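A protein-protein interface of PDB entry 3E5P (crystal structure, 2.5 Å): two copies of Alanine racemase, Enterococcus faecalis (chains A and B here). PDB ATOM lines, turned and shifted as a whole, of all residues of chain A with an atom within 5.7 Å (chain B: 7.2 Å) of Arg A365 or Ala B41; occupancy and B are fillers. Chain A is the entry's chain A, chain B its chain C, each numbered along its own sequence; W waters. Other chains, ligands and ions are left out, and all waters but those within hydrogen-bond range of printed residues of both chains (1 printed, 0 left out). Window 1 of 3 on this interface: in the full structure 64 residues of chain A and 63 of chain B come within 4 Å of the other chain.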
ATOM      1  N   VAL A   2       3.993   1.790 -24.484  1.00  0.00           N
ATOM      2  CA  VAL A   2       3.109   0.965 -23.615  1.00  0.00           C
ATOM      3  C   VAL A   2       2.700  -0.355 -24.244  1.00  0.00           C
ATOM      4  O   VAL A   2       2.058  -0.383 -25.286  1.00  0.00           O
ATOM      5  CB  VAL A   2       1.827   1.716 -23.263  1.00  0.00           C
ATOM      6  CG1 VAL A   2       0.865   0.794 -22.549  1.00  0.00           C
ATOM      7  CG2 VAL A   2       2.150   2.911 -22.392  1.00  0.00           C
ATOM      8  N   VAL A   3       3.063  -1.451 -23.591  1.00  0.00           N
ATOM      9  CA  VAL A   3       2.711  -2.783 -24.064  1.00  0.00           C
ATOM     10  C   VAL A   3       1.479  -3.278 -23.292  1.00  0.00           C
ATOM     11  O   VAL A   3       1.490  -3.331 -22.070  1.00  0.00           O
ATOM     12  CB  VAL A   3       3.884  -3.740 -23.839  1.00  0.00           C
ATOM     13  CG1 VAL A   3       3.532  -5.136 -24.314  1.00  0.00           C
ATOM     14  CG2 VAL A   3       5.088  -3.218 -24.564  1.00  0.00           C
ATOM     15  N   GLY A   4       0.418  -3.643 -23.999  1.00  0.00           N
ATOM     16  CA  GLY A   4      -0.786  -4.092 -23.321  1.00  0.00           C
ATOM     17  C   GLY A   4      -0.758  -5.503 -22.765  1.00  0.00           C
ATOM     18  O   GLY A   4      -1.599  -6.329 -23.110  1.00  0.00           O
ATOM     19  N   TRP A   5       0.197  -5.786 -21.888  1.00  0.00           N
ATOM     20  CA  TRP A   5       0.307  -7.115 -21.286  1.00  0.00           C
ATOM     21  C   TRP A   5      -0.938  -7.573 -20.528  1.00  0.00           C
ATOM     22  O   TRP A   5      -1.174  -8.767 -20.397  1.00  0.00           O
ATOM     23  CB  TRP A   5       1.515  -7.166 -20.339  1.00  0.00           C
ATOM     24  CG  TRP A   5       2.823  -7.299 -21.047  1.00  0.00           C
ATOM     25  CD1 TRP A   5       3.793  -6.335 -21.195  1.00  0.00           C
ATOM     26  CD2 TRP A   5       3.279  -8.443 -21.775  1.00  0.00           C
ATOM     27  NE1 TRP A   5       4.817  -6.814 -21.977  1.00  0.00           N
ATOM     28  CE2 TRP A   5       4.529  -8.104 -22.346  1.00  0.00           C
ATOM     29  CE3 TRP A   5       2.749  -9.724 -22.005  1.00  0.00           C
ATOM     30  CZ2 TRP A   5       5.255  -8.998 -23.133  1.00  0.00           C
ATOM     31  CZ3 TRP A   5       3.476 -10.619 -22.791  1.00  0.00           C
ATOM     32  CH2 TRP A   5       4.712 -10.249 -23.344  1.00  0.00           C
ATOM     33  N   ARG A   7      -4.043  -6.946 -21.408  1.00  0.00           N
ATOM     34  CA  ARG A   7      -5.189  -7.075 -22.290  1.00  0.00           C
ATOM     35  C   ARG A   7      -5.114  -8.440 -22.937  1.00  0.00           C
ATOM     36  O   ARG A   7      -4.061  -8.859 -23.390  1.00  0.00           O
ATOM     37  CB  ARG A   7      -5.167  -5.982 -23.348  1.00  0.00           C
ATOM     38  CG  ARG A   7      -6.307  -6.056 -24.328  1.00  0.00           C
ATOM     39  CD  ARG A   7      -6.232  -4.930 -25.337  1.00  0.00           C
ATOM     40  NE  ARG A   7      -4.947  -4.875 -26.023  1.00  0.00           N
ATOM     41  CZ  ARG A   7      -4.735  -4.166 -27.124  1.00  0.00           C
ATOM     42  NH1 ARG A   7      -5.729  -3.462 -27.654  1.00  0.00           N
ATOM     43  NH2 ARG A   7      -3.535  -4.152 -27.698  1.00  0.00           N
ATOM     44  N   ILE A 284      -9.439  -4.930 -29.547  1.00  0.00           N
ATOM     45  CA  ILE A 284      -8.437  -4.642 -30.567  1.00  0.00           C
ATOM     46  C   ILE A 284      -9.074  -3.790 -31.655  1.00  0.00           C
ATOM     47  O   ILE A 284     -10.126  -4.145 -32.189  1.00  0.00           O
ATOM     48  CB  ILE A 284      -7.898  -5.928 -31.235  1.00  0.00           C
ATOM     49  CG1 ILE A 284      -6.796  -5.575 -32.242  1.00  0.00           C
ATOM     50  CG2 ILE A 284      -9.037  -6.672 -31.925  1.00  0.00           C
ATOM     51  CD1 ILE A 284      -6.226  -6.772 -32.969  1.00  0.00           C
ATOM     52  N   GLY A 285      -8.434  -2.672 -31.986  1.00  0.00           N
ATOM     53  CA  GLY A 285      -8.968  -1.793 -33.009  1.00  0.00           C
ATOM     54  C   GLY A 285      -7.885  -1.307 -33.943  1.00  0.00           C
ATOM     55  O   GLY A 285      -6.811  -1.902 -34.000  1.00  0.00           O
ATOM     56  N   ALA A 287      -5.978   1.248 -33.710  1.00  0.00           N
ATOM     57  CA  ALA A 287      -4.816   1.783 -33.003  1.00  0.00           C
ATOM     58  C   ALA A 287      -3.807   0.657 -32.753  1.00  0.00           C
ATOM     59  O   ALA A 287      -2.701   0.904 -32.287  1.00  0.00           O
ATOM     60  CB  ALA A 287      -5.242   2.406 -31.680  1.00  0.00           C
ATOM     61  N   ASP A 288      -4.195  -0.581 -33.055  1.00  0.00           N
ATOM     62  CA  ASP A 288      -3.291  -1.724 -32.890  1.00  0.00           C
ATOM     63  C   ASP A 288      -2.824  -2.175 -34.268  1.00  0.00           C
ATOM     64  O   ASP A 288      -1.971  -3.058 -34.405  1.00  0.00           O
ATOM     65  CB  ASP A 288      -3.995  -2.902 -32.192  1.00  0.00           C
ATOM     66  CG  ASP A 288      -4.427  -2.574 -30.768  1.00  0.00           C
ATOM     67  OD1 ASP A 288      -3.610  -2.043 -29.978  1.00  0.00           O
ATOM     68  OD2 ASP A 288      -5.594  -2.859 -30.437  1.00  0.00           O
ATOM     69  N   MET A 314     -11.096   2.609 -32.374  1.00  0.00           N
ATOM     70  CA  MET A 314      -9.680   2.768 -32.138  1.00  0.00           C
ATOM     71  C   MET A 314      -9.159   1.607 -31.292  1.00  0.00           C
ATOM     72  O   MET A 314      -8.089   1.081 -31.562  1.00  0.00           O
ATOM     73  CB  MET A 314      -9.410   4.087 -31.417  1.00  0.00           C
ATOM     74  CG  MET A 314      -7.947   4.370 -31.176  1.00  0.00           C
ATOM     75  SD  MET A 314      -7.691   5.972 -30.400  1.00  0.00           S
ATOM     76  CE  MET A 314      -8.629   7.056 -31.512  1.00  0.00           C
ATOM     77  N   ASP A 315      -9.920   1.190 -30.289  1.00  0.00           N
ATOM     78  CA  ASP A 315      -9.447   0.125 -29.415  1.00  0.00           C
ATOM     79  C   ASP A 315     -10.160  -1.211 -29.452  1.00  0.00           C
ATOM     80  O   ASP A 315      -9.728  -2.163 -28.804  1.00  0.00           O
ATOM     81  CB  ASP A 315      -9.398   0.640 -27.985  1.00  0.00           C
ATOM     82  CG  ASP A 315      -8.529   1.866 -27.856  1.00  0.00           C
ATOM     83  OD1 ASP A 315      -7.322   1.758 -28.170  1.00  0.00           O
ATOM     84  OD2 ASP A 315      -9.050   2.933 -27.455  1.00  0.00           O
ATOM     85  N   SER A 363       0.844  -2.577 -34.097  1.00  0.00           N
ATOM     86  CA  SER A 363       1.312  -1.718 -33.026  1.00  0.00           C
ATOM     87  C   SER A 363       2.189  -2.342 -31.962  1.00  0.00           C
ATOM     88  O   SER A 363       2.085  -3.525 -31.646  1.00  0.00           O
ATOM     89  CB  SER A 363       0.118  -1.068 -32.337  1.00  0.00           C
ATOM     90  OG  SER A 363       0.543  -0.132 -31.365  1.00  0.00           O
ATOM     91  N   GLN A 364       3.053  -1.505 -31.408  1.00  0.00           N
ATOM     92  CA  GLN A 364       3.964  -1.894 -30.353  1.00  0.00           C
ATOM     93  C   GLN A 364       3.093  -2.291 -29.153  1.00  0.00           C
ATOM     94  O   GLN A 364       3.519  -3.053 -28.284  1.00  0.00           O
ATOM     95  CB  GLN A 364       4.853  -0.689 -29.998  1.00  0.00           C
ATOM     96  CG  GLN A 364       5.849  -0.893 -28.850  1.00  0.00           C
ATOM     97  CD  GLN A 364       6.195   0.418 -28.115  1.00  0.00           C
ATOM     98  OE1 GLN A 364       5.422   0.907 -27.279  1.00  0.00           O
ATOM     99  NE2 GLN A 364       7.352   0.992 -28.439  1.00  0.00           N
ATOM    100  N   ARG A 365       1.864  -1.780 -29.135  1.00  0.00           N
ATOM    101  CA  ARG A 365       0.933  -2.037 -28.048  1.00  0.00           C
ATOM    102  C   ARG A 365       0.485  -3.497 -27.916  1.00  0.00           C
ATOM    103  O   ARG A 365      -0.082  -3.895 -26.894  1.00  0.00           O
ATOM    104  CB  ARG A 365      -0.286  -1.123 -28.190  1.00  0.00           C
ATOM    105  CG  ARG A 365      -1.098  -0.997 -26.921  1.00  0.00           C
ATOM    106  CD  ARG A 365      -2.186   0.046 -27.042  1.00  0.00           C
ATOM    107  NE  ARG A 365      -3.224  -0.372 -27.971  1.00  0.00           N
ATOM    108  CZ  ARG A 365      -4.373   0.269 -28.140  1.00  0.00           C
ATOM    109  NH1 ARG A 365      -4.624   1.362 -27.441  1.00  0.00           N
ATOM    110  NH2 ARG A 365      -5.274  -0.194 -28.998  1.00  0.00           N
ATOM    111  N   ILE A 366       0.741  -4.297 -28.941  1.00  0.00           N
ATOM    112  CA  ILE A 366       0.361  -5.702 -28.901  1.00  0.00           C
ATOM    113  C   ILE A 366       1.583  -6.529 -28.484  1.00  0.00           C
ATOM    114  O   ILE A 366       2.574  -6.600 -29.213  1.00  0.00           O
ATOM    115  CB  ILE A 366      -0.156  -6.174 -30.277  1.00  0.00           C
ATOM    116  CG1 ILE A 366      -1.243  -5.212 -30.783  1.00  0.00           C
ATOM    117  CG2 ILE A 366      -0.729  -7.563 -30.162  1.00  0.00           C
ATOM    118  CD1 ILE A 366      -1.931  -5.641 -32.071  1.00  0.00           C
ATOM    119  N   PRO A 367       1.533  -7.147 -27.293  1.00  0.00           N
ATOM    120  CA  PRO A 367       2.642  -7.962 -26.788  1.00  0.00           C
ATOM    121  C   PRO A 367       2.992  -9.141 -27.684  1.00  0.00           C
ATOM    122  O   PRO A 367       2.127  -9.927 -28.051  1.00  0.00           O
ATOM    123  CB  PRO A 367       2.135  -8.434 -25.423  1.00  0.00           C
ATOM    124  CG  PRO A 367       1.224  -7.336 -24.999  1.00  0.00           C
ATOM    125  CD  PRO A 367       0.477  -7.023 -26.275  1.00  0.00           C
ATOM    126  N   ARG A 368       4.260  -9.258 -28.050  1.00  0.00           N
ATOM    127  CA  ARG A 368       4.690 -10.385 -28.856  1.00  0.00           C
ATOM    128  C   ARG A 368       5.163 -11.473 -27.890  1.00  0.00           C
ATOM    129  O   ARG A 368       5.927 -11.188 -26.971  1.00  0.00           O
ATOM    130  CB  ARG A 368       5.852  -9.995 -29.765  1.00  0.00           C
ATOM    131  CG  ARG A 368       5.473  -9.389 -31.099  1.00  0.00           C
ATOM    132  CD  ARG A 368       5.166  -7.895 -31.022  1.00  0.00           C
ATOM    133  NE  ARG A 368       4.968  -7.350 -32.364  1.00  0.00           N
ATOM    134  CZ  ARG A 368       4.427  -6.165 -32.618  1.00  0.00           C
ATOM    135  NH1 ARG A 368       4.038  -5.405 -31.619  1.00  0.00           N
ATOM    136  NH2 ARG A 368       4.256  -5.748 -33.863  1.00  0.00           N
ATOM    137  N   VAL B  38      -8.902  12.604 -22.765  1.00  0.00           N
ATOM    138  CA  VAL B  38      -8.738  11.197 -23.110  1.00  0.00           C
ATOM    139  C   VAL B  38      -7.452  11.085 -23.924  1.00  0.00           C
ATOM    140  O   VAL B  38      -7.320  11.694 -24.984  1.00  0.00           O
ATOM    141  CB  VAL B  38      -9.951  10.655 -23.910  1.00  0.00           C
ATOM    142  CG1 VAL B  38     -10.363  11.636 -24.953  1.00  0.00           C
ATOM    143  CG2 VAL B  38      -9.606   9.340 -24.566  1.00  0.00           C
ATOM    144  N   VAL B  39      -6.284  10.346 -23.367  1.00  0.00           N
ATOM    145  CA  VAL B  39      -5.005  10.203 -24.037  1.00  0.00           C
ATOM    146  C   VAL B  39      -4.675   8.760 -24.373  1.00  0.00           C
ATOM    147  O   VAL B  39      -3.515   8.339 -24.281  1.00  0.00           O
ATOM    148  CB  VAL B  39      -3.864  10.790 -23.171  1.00  0.00           C
ATOM    149  CG1 VAL B  39      -4.091  12.283 -22.971  1.00  0.00           C
ATOM    150  CG2 VAL B  39      -3.795  10.071 -21.822  1.00  0.00           C
ATOM    151  N   LYS B  40      -5.691   7.998 -24.766  1.00  0.00           N
ATOM    152  CA  LYS B  40      -5.507   6.592 -25.106  1.00  0.00           C
ATOM    153  C   LYS B  40      -4.625   6.431 -26.341  1.00  0.00           C
ATOM    154  O   LYS B  40      -4.414   7.384 -27.091  1.00  0.00           O
ATOM    155  CB  LYS B  40      -6.860   5.914 -25.333  1.00  0.00           C
ATOM    156  CG  LYS B  40      -7.733   6.601 -26.370  1.00  0.00           C
ATOM    157  CD  LYS B  40      -8.974   5.780 -26.678  1.00  0.00           C
ATOM    158  CE  LYS B  40      -9.882   6.499 -27.664  1.00  0.00           C
ATOM    159  NZ  LYS B  40     -10.456   7.743 -27.084  1.00  0.00           N
ATOM    160  N   ALA B  41      -4.326   5.201 -26.583  1.00  0.00           N
ATOM    161  CA  ALA B  41      -3.493   4.909 -27.739  1.00  0.00           C
ATOM    162  C   ALA B  41      -2.336   5.898 -27.805  1.00  0.00           C
ATOM    163  O   ALA B  41      -2.108   6.543 -28.835  1.00  0.00           O
ATOM    164  CB  ALA B  41      -4.325   4.983 -29.026  1.00  0.00           C
ATOM    165  N   ASN B  42      -1.609   5.997 -26.694  1.00  0.00           N
ATOM    166  CA  ASN B  42      -0.461   6.883 -26.570  1.00  0.00           C
ATOM    167  C   ASN B  42      -0.824   8.291 -27.016  1.00  0.00           C
ATOM    168  O   ASN B  42      -0.153   8.883 -27.856  1.00  0.00           O
ATOM    169  CB  ASN B  42       0.715   6.335 -27.391  1.00  0.00           C
ATOM    170  CG  ASN B  42       2.057   6.923 -26.960  1.00  0.00           C
ATOM    171  OD1 ASN B  42       2.278   7.195 -25.775  1.00  0.00           O
ATOM    172  ND2 ASN B  42       2.965   7.100 -27.916  1.00  0.00           N
ATOM    173  N   GLY B  43      -1.893   8.826 -26.436  1.00  0.00           N
ATOM    174  CA  GLY B  43      -2.333  10.157 -26.794  1.00  0.00           C
ATOM    175  C   GLY B  43      -2.581  10.225 -28.288  1.00  0.00           C
ATOM    176  O   GLY B  43      -2.053  11.106 -28.973  1.00  0.00           O
ATOM    177  N   TYR B  44      -3.376   9.287 -28.801  1.00  0.00           N
ATOM    178  CA  TYR B  44      -3.671   9.253 -30.224  1.00  0.00           C
ATOM    179  C   TYR B  44      -2.389   9.390 -31.036  1.00  0.00           C
ATOM    180  O   TYR B  44      -2.349  10.117 -32.034  1.00  0.00           O
ATOM    181  CB  TYR B  44      -4.630  10.386 -30.602  1.00  0.00           C
ATOM    182  CG  TYR B  44      -6.005  10.252 -29.985  1.00  0.00           C
ATOM    183  CD1 TYR B  44      -6.152   9.980 -28.622  1.00  0.00           C
ATOM    184  CD2 TYR B  44      -7.155  10.438 -30.749  1.00  0.00           C
ATOM    185  CE1 TYR B  44      -7.401   9.896 -28.036  1.00  0.00           C
ATOM    186  CE2 TYR B  44      -8.415  10.362 -30.170  1.00  0.00           C
ATOM    187  CZ  TYR B  44      -8.531  10.089 -28.807  1.00  0.00           C
ATOM    188  OH  TYR B  44      -9.771  10.003 -28.210  1.00  0.00           O
ATOM    189  N   GLY B  45      -1.341   8.709 -30.584  1.00  0.00           N
ATOM    190  CA  GLY B  45      -0.078   8.739 -31.297  1.00  0.00           C
ATOM    191  C   GLY B  45       0.850   9.910 -31.031  1.00  0.00           C
ATOM    192  O   GLY B  45       1.950   9.966 -31.586  1.00  0.00           O
ATOM    193  N   HIS B  46       0.418  10.846 -30.198  1.00  0.00           N
ATOM    194  CA  HIS B  46       1.254  11.998 -29.892  1.00  0.00           C
ATOM    195  C   HIS B  46       2.084  11.765 -28.630  1.00  0.00           C
ATOM    196  O   HIS B  46       3.044  12.496 -28.376  1.00  0.00           O
ATOM    197  CB  HIS B  46       0.402  13.254 -29.683  1.00  0.00           C
ATOM    198  CG  HIS B  46      -0.435  13.629 -30.863  1.00  0.00           C
ATOM    199  ND1 HIS B  46      -1.453  12.829 -31.338  1.00  0.00           N
ATOM    200  CD2 HIS B  46      -0.455  14.753 -31.619  1.00  0.00           C
ATOM    201  CE1 HIS B  46      -2.069  13.447 -32.333  1.00  0.00           C
ATOM    202  NE2 HIS B  46      -1.484  14.617 -32.521  1.00  0.00           N
ATOM    203  N   GLY B  47       1.707  10.754 -27.849  1.00  0.00           N
ATOM    204  CA  GLY B  47       2.404  10.457 -26.610  1.00  0.00           C
ATOM    205  C   GLY B  47       1.522  10.835 -25.433  1.00  0.00           C
ATOM    206  O   GLY B  47       1.288  12.024 -25.172  1.00  0.00           O
ATOM    207  N   ALA B  48       1.041   9.823 -24.713  1.00  0.00           N
ATOM    208  CA  ALA B  48       0.145  10.032 -23.576  1.00  0.00           C
ATOM    209  C   ALA B  48       0.638  11.001 -22.508  1.00  0.00           C
ATOM    210  O   ALA B  48       0.064  12.077 -22.335  1.00  0.00           O
ATOM    211  CB  ALA B  48      -0.189   8.698 -22.940  1.00  0.00           C
ATOM    212  N   CYS B  64      -8.915   9.984 -19.484  1.00  0.00           N
ATOM    213  CA  CYS B  64      -9.610   8.830 -20.041  1.00  0.00           C
ATOM    214  C   CYS B  64      -8.642   7.978 -20.834  1.00  0.00           C
ATOM    215  O   CYS B  64      -8.065   8.427 -21.830  1.00  0.00           O
ATOM    216  CB  CYS B  64     -10.732   9.274 -20.962  1.00  0.00           C
ATOM    217  SG  CYS B  64     -12.105   9.972 -20.091  1.00  0.00           S
ATOM    218  N   VAL B  65      -8.484   6.739 -20.389  1.00  0.00           N
ATOM    219  CA  VAL B  65      -7.574   5.809 -21.023  1.00  0.00           C
ATOM    220  C   VAL B  65      -8.360   4.586 -21.481  1.00  0.00           C
ATOM    221  O   VAL B  65      -9.507   4.398 -21.070  1.00  0.00           O
ATOM    222  CB  VAL B  65      -6.488   5.408 -20.022  1.00  0.00           C
ATOM    223  CG1 VAL B  65      -6.748   4.000 -19.488  1.00  0.00           C
ATOM    224  CG2 VAL B  65      -5.142   5.558 -20.650  1.00  0.00           C
ATOM    225  N   ALA B  66      -7.739   3.755 -22.318  1.00  0.00           N
ATOM    226  CA  ALA B  66      -8.389   2.565 -22.852  1.00  0.00           C
ATOM    227  C   ALA B  66      -7.900   1.243 -22.256  1.00  0.00           C
ATOM    228  O   ALA B  66      -8.612   0.241 -22.284  1.00  0.00           O
ATOM    229  CB  ALA B  66      -8.217   2.534 -24.353  1.00  0.00           C
ATOM    230  N   LEU B  67      -6.684   1.221 -21.733  1.00  0.00           N
ATOM    231  CA  LEU B  67      -6.175  -0.014 -21.156  1.00  0.00           C
ATOM    232  C   LEU B  67      -5.701   0.166 -19.725  1.00  0.00           C
ATOM    233  O   LEU B  67      -5.368   1.270 -19.313  1.00  0.00           O
ATOM    234  CB  LEU B  67      -5.006  -0.556 -21.985  1.00  0.00           C
ATOM    235  CG  LEU B  67      -5.144  -0.724 -23.501  1.00  0.00           C
ATOM    236  CD1 LEU B  67      -4.061  -1.691 -23.986  1.00  0.00           C
ATOM    237  CD2 LEU B  67      -6.516  -1.264 -23.848  1.00  0.00           C
ATOM    238  N   ASP B  69      -2.972  -1.019 -18.564  1.00  0.00           N
ATOM    239  CA  ASP B  69      -1.570  -0.672 -18.750  1.00  0.00           C
ATOM    240  C   ASP B  69      -1.360   0.809 -19.081  1.00  0.00           C
ATOM    241  O   ASP B  69      -0.332   1.391 -18.737  1.00  0.00           O
ATOM    242  CB  ASP B  69      -0.979  -1.539 -19.865  1.00  0.00           C
ATOM    243  CG  ASP B  69      -0.939  -3.020 -19.495  1.00  0.00           C
ATOM    244  OD1 ASP B  69      -0.206  -3.353 -18.535  1.00  0.00           O
ATOM    245  OD2 ASP B  69      -1.632  -3.845 -20.148  1.00  0.00           O
ATOM    246  N   GLU B  70      -2.331   1.424 -19.748  1.00  0.00           N
ATOM    247  CA  GLU B  70      -2.204   2.832 -20.105  1.00  0.00           C
ATOM    248  C   GLU B  70      -2.507   3.718 -18.909  1.00  0.00           C
ATOM    249  O   GLU B  70      -1.909   4.789 -18.748  1.00  0.00           O
ATOM    250  CB  GLU B  70      -3.136   3.179 -21.271  1.00  0.00           C
ATOM    251  CG  GLU B  70      -2.687   2.615 -22.612  1.00  0.00           C
ATOM    252  CD  GLU B  70      -3.733   2.787 -23.709  1.00  0.00           C
ATOM    253  OE1 GLU B  70      -3.447   2.415 -24.866  1.00  0.00           O
ATOM    254  OE2 GLU B  70      -4.842   3.286 -23.415  1.00  0.00           O
ATOM    255  N   TYR B 228      -6.058  17.673 -29.942  1.00  0.00           N
ATOM    256  CA  TYR B 228      -4.827  17.546 -30.708  1.00  0.00           C
ATOM    257  C   TYR B 228      -4.967  18.413 -31.970  1.00  0.00           C
ATOM    258  O   TYR B 228      -4.169  18.322 -32.911  1.00  0.00           O
ATOM    259  CB  TYR B 228      -4.593  16.095 -31.087  1.00  0.00           C
ATOM    260  CG  TYR B 228      -4.622  15.154 -29.913  1.00  0.00           C
ATOM    261  CD1 TYR B 228      -3.534  15.047 -29.042  1.00  0.00           C
ATOM    262  CD2 TYR B 228      -5.746  14.367 -29.668  1.00  0.00           C
ATOM    263  CE1 TYR B 228      -3.565  14.178 -27.954  1.00  0.00           C
ATOM    264  CE2 TYR B 228      -5.795  13.492 -28.578  1.00  0.00           C
ATOM    265  CZ  TYR B 228      -4.701  13.402 -27.729  1.00  0.00           C
ATOM    266  OH  TYR B 228      -4.747  12.512 -26.684  1.00  0.00           O
ATOM    267  N   ALA B 359      -2.913   9.139 -37.367  1.00  0.00           N
ATOM    268  CA  ALA B 359      -2.082   9.497 -36.226  1.00  0.00           C
ATOM    269  C   ALA B 359      -1.704   8.275 -35.400  1.00  0.00           C
ATOM    270  O   ALA B 359      -0.582   8.170 -34.931  1.00  0.00           O
ATOM    271  CB  ALA B 359      -2.800  10.513 -35.354  1.00  0.00           C
ATOM    272  N   CYS B 360      -2.636   7.353 -35.222  1.00  0.00           N
ATOM    273  CA  CYS B 360      -2.344   6.156 -34.451  1.00  0.00           C
ATOM    274  C   CYS B 360      -1.458   5.166 -35.193  1.00  0.00           C
ATOM    275  O   CYS B 360      -0.907   4.250 -34.589  1.00  0.00           O
ATOM    276  CB  CYS B 360      -3.639   5.446 -34.047  1.00  0.00           C
ATOM    277  SG  CYS B 360      -4.632   6.364 -32.872  1.00  0.00           S
ATOM    278  N   ARG B 368       9.558  11.172 -31.479  1.00  0.00           N
ATOM    279  CA  ARG B 368       8.672  12.302 -31.255  1.00  0.00           C
ATOM    280  C   ARG B 368       9.390  13.337 -30.394  1.00  0.00           C
ATOM    281  O   ARG B 368       9.980  12.993 -29.369  1.00  0.00           O
ATOM    282  CB  ARG B 368       7.408  11.872 -30.523  1.00  0.00           C
ATOM    283  CG  ARG B 368       6.303  11.376 -31.393  1.00  0.00           C
ATOM    284  CD  ARG B 368       6.377   9.891 -31.635  1.00  0.00           C
ATOM    285  NE  ARG B 368       5.051   9.398 -31.988  1.00  0.00           N
ATOM    286  CZ  ARG B 368       4.803   8.172 -32.417  1.00  0.00           C
ATOM    287  NH1 ARG B 368       5.793   7.306 -32.544  1.00  0.00           N
ATOM    288  NH2 ARG B 368       3.566   7.820 -32.739  1.00  0.00           N
HETATM  289  O   HOH W   1      -0.752   2.834 -32.337  1.00  0.00           O
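Position printed for both chains: 368.
Water W1 lies within hydrogen-bond range of the backbone carbonyl oxygen of Cys B360 (2.7 Å), the backbone carbonyl oxygen of Ala A287 (2.7 Å) and the side-chain hydroxyl of Ser A363 (3.4 Å).
Of the printed residues of chain B, Arg A365 touches Ala B41 (3.7 Å), Leu B67 (3.98 Å) and Glu B70 (3.0 Å).
Ala B41 touches just these residues of chain A: Ala A287, Met A314 and Arg A365.
Of the printed residues of chain A, Asp B69 touches Val A3 (3.6 Å), Gly A4 (3.2 Å) and Trp A5 (3.2 Å).
Of the printed residues of chain A, Lys B40 touches Met A314 and Asp A315.
Of the printed residues of chain B, Val A3 touches Asp B69 (3.6 Å).
Asn B42 touches none of the printed residues of chain A.
Val B39 touches none of the printed residues of chain A.
The backbone NH (N) of Trp A5 sits at hydrogen-bond distance from the side-chain carboxylate (OD2) of Asp B69, at 3.2 Å.
OE1 of Glu B70 is in salt-bridge range of NH1 of Arg A365 (3.0 Å).
Of the 21 printed residues of chain B, 8 touch a printed residue of chain A.
Hydrophobic or aromatic side chains of chain B within 4 Å of the printed part of chain A: Ala B41, Tyr B44, Ala B66 and Leu B67.
Hydrophobic or aromatic side chains of chain A that line the printed part of chain B: Val A2, Ala A287 and Met A314.
Along chain A the printed residues that touch a printed residue of chain B span positions 2 to 365.
Among the printed residues, 16 pairs touch across the chains.
Among the printed residues, Asp or Glu carboxylates within 4 Å of a Lys or Arg side-chain nitrogen of the other chain: Arg A365 with Glu B70 (3.0 Å).
The backbone NH (N) of Val A2 is in hydrogen-bond range of the side-chain amide oxygen (OE1) of Gln A364 (3.3 Å).
N of Ile A284 lies within hydrogen-bond range of O of Asp A315 (2.9 Å).
NE of Arg A365 is in salt-bridge range of OD1 of Asp A288.
OD1 of Asp A315 is in salt-bridge range of NH1 of Arg A365 (2.8 Å).
The side-chain hydroxyl (OG) of Ser A363 lies close to the backbone NH (N) of Arg A365 (3.1 Å).
NZ of Lys B40 lies within hydrogen-bond range of OH of Tyr B44 (2.6 Å).
Among the printed residues, merely in contact across the chains: Val A2 with Glu B70, Val A3 with Asp B69, Gly A4 with Asp B69, Arg A7 with Leu B67, Ala A287 with Ala B41, Ala A287 with Cys B360, Met A314 with Lys B40, Met A314 with Ala B41, Met A314 with Tyr B44, Met A314 with Cys B360, Asp A315 with Lys B40, Asp A315 with Ala B66, Arg A365 with Ala B41 and Arg A365 with Leu B67.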
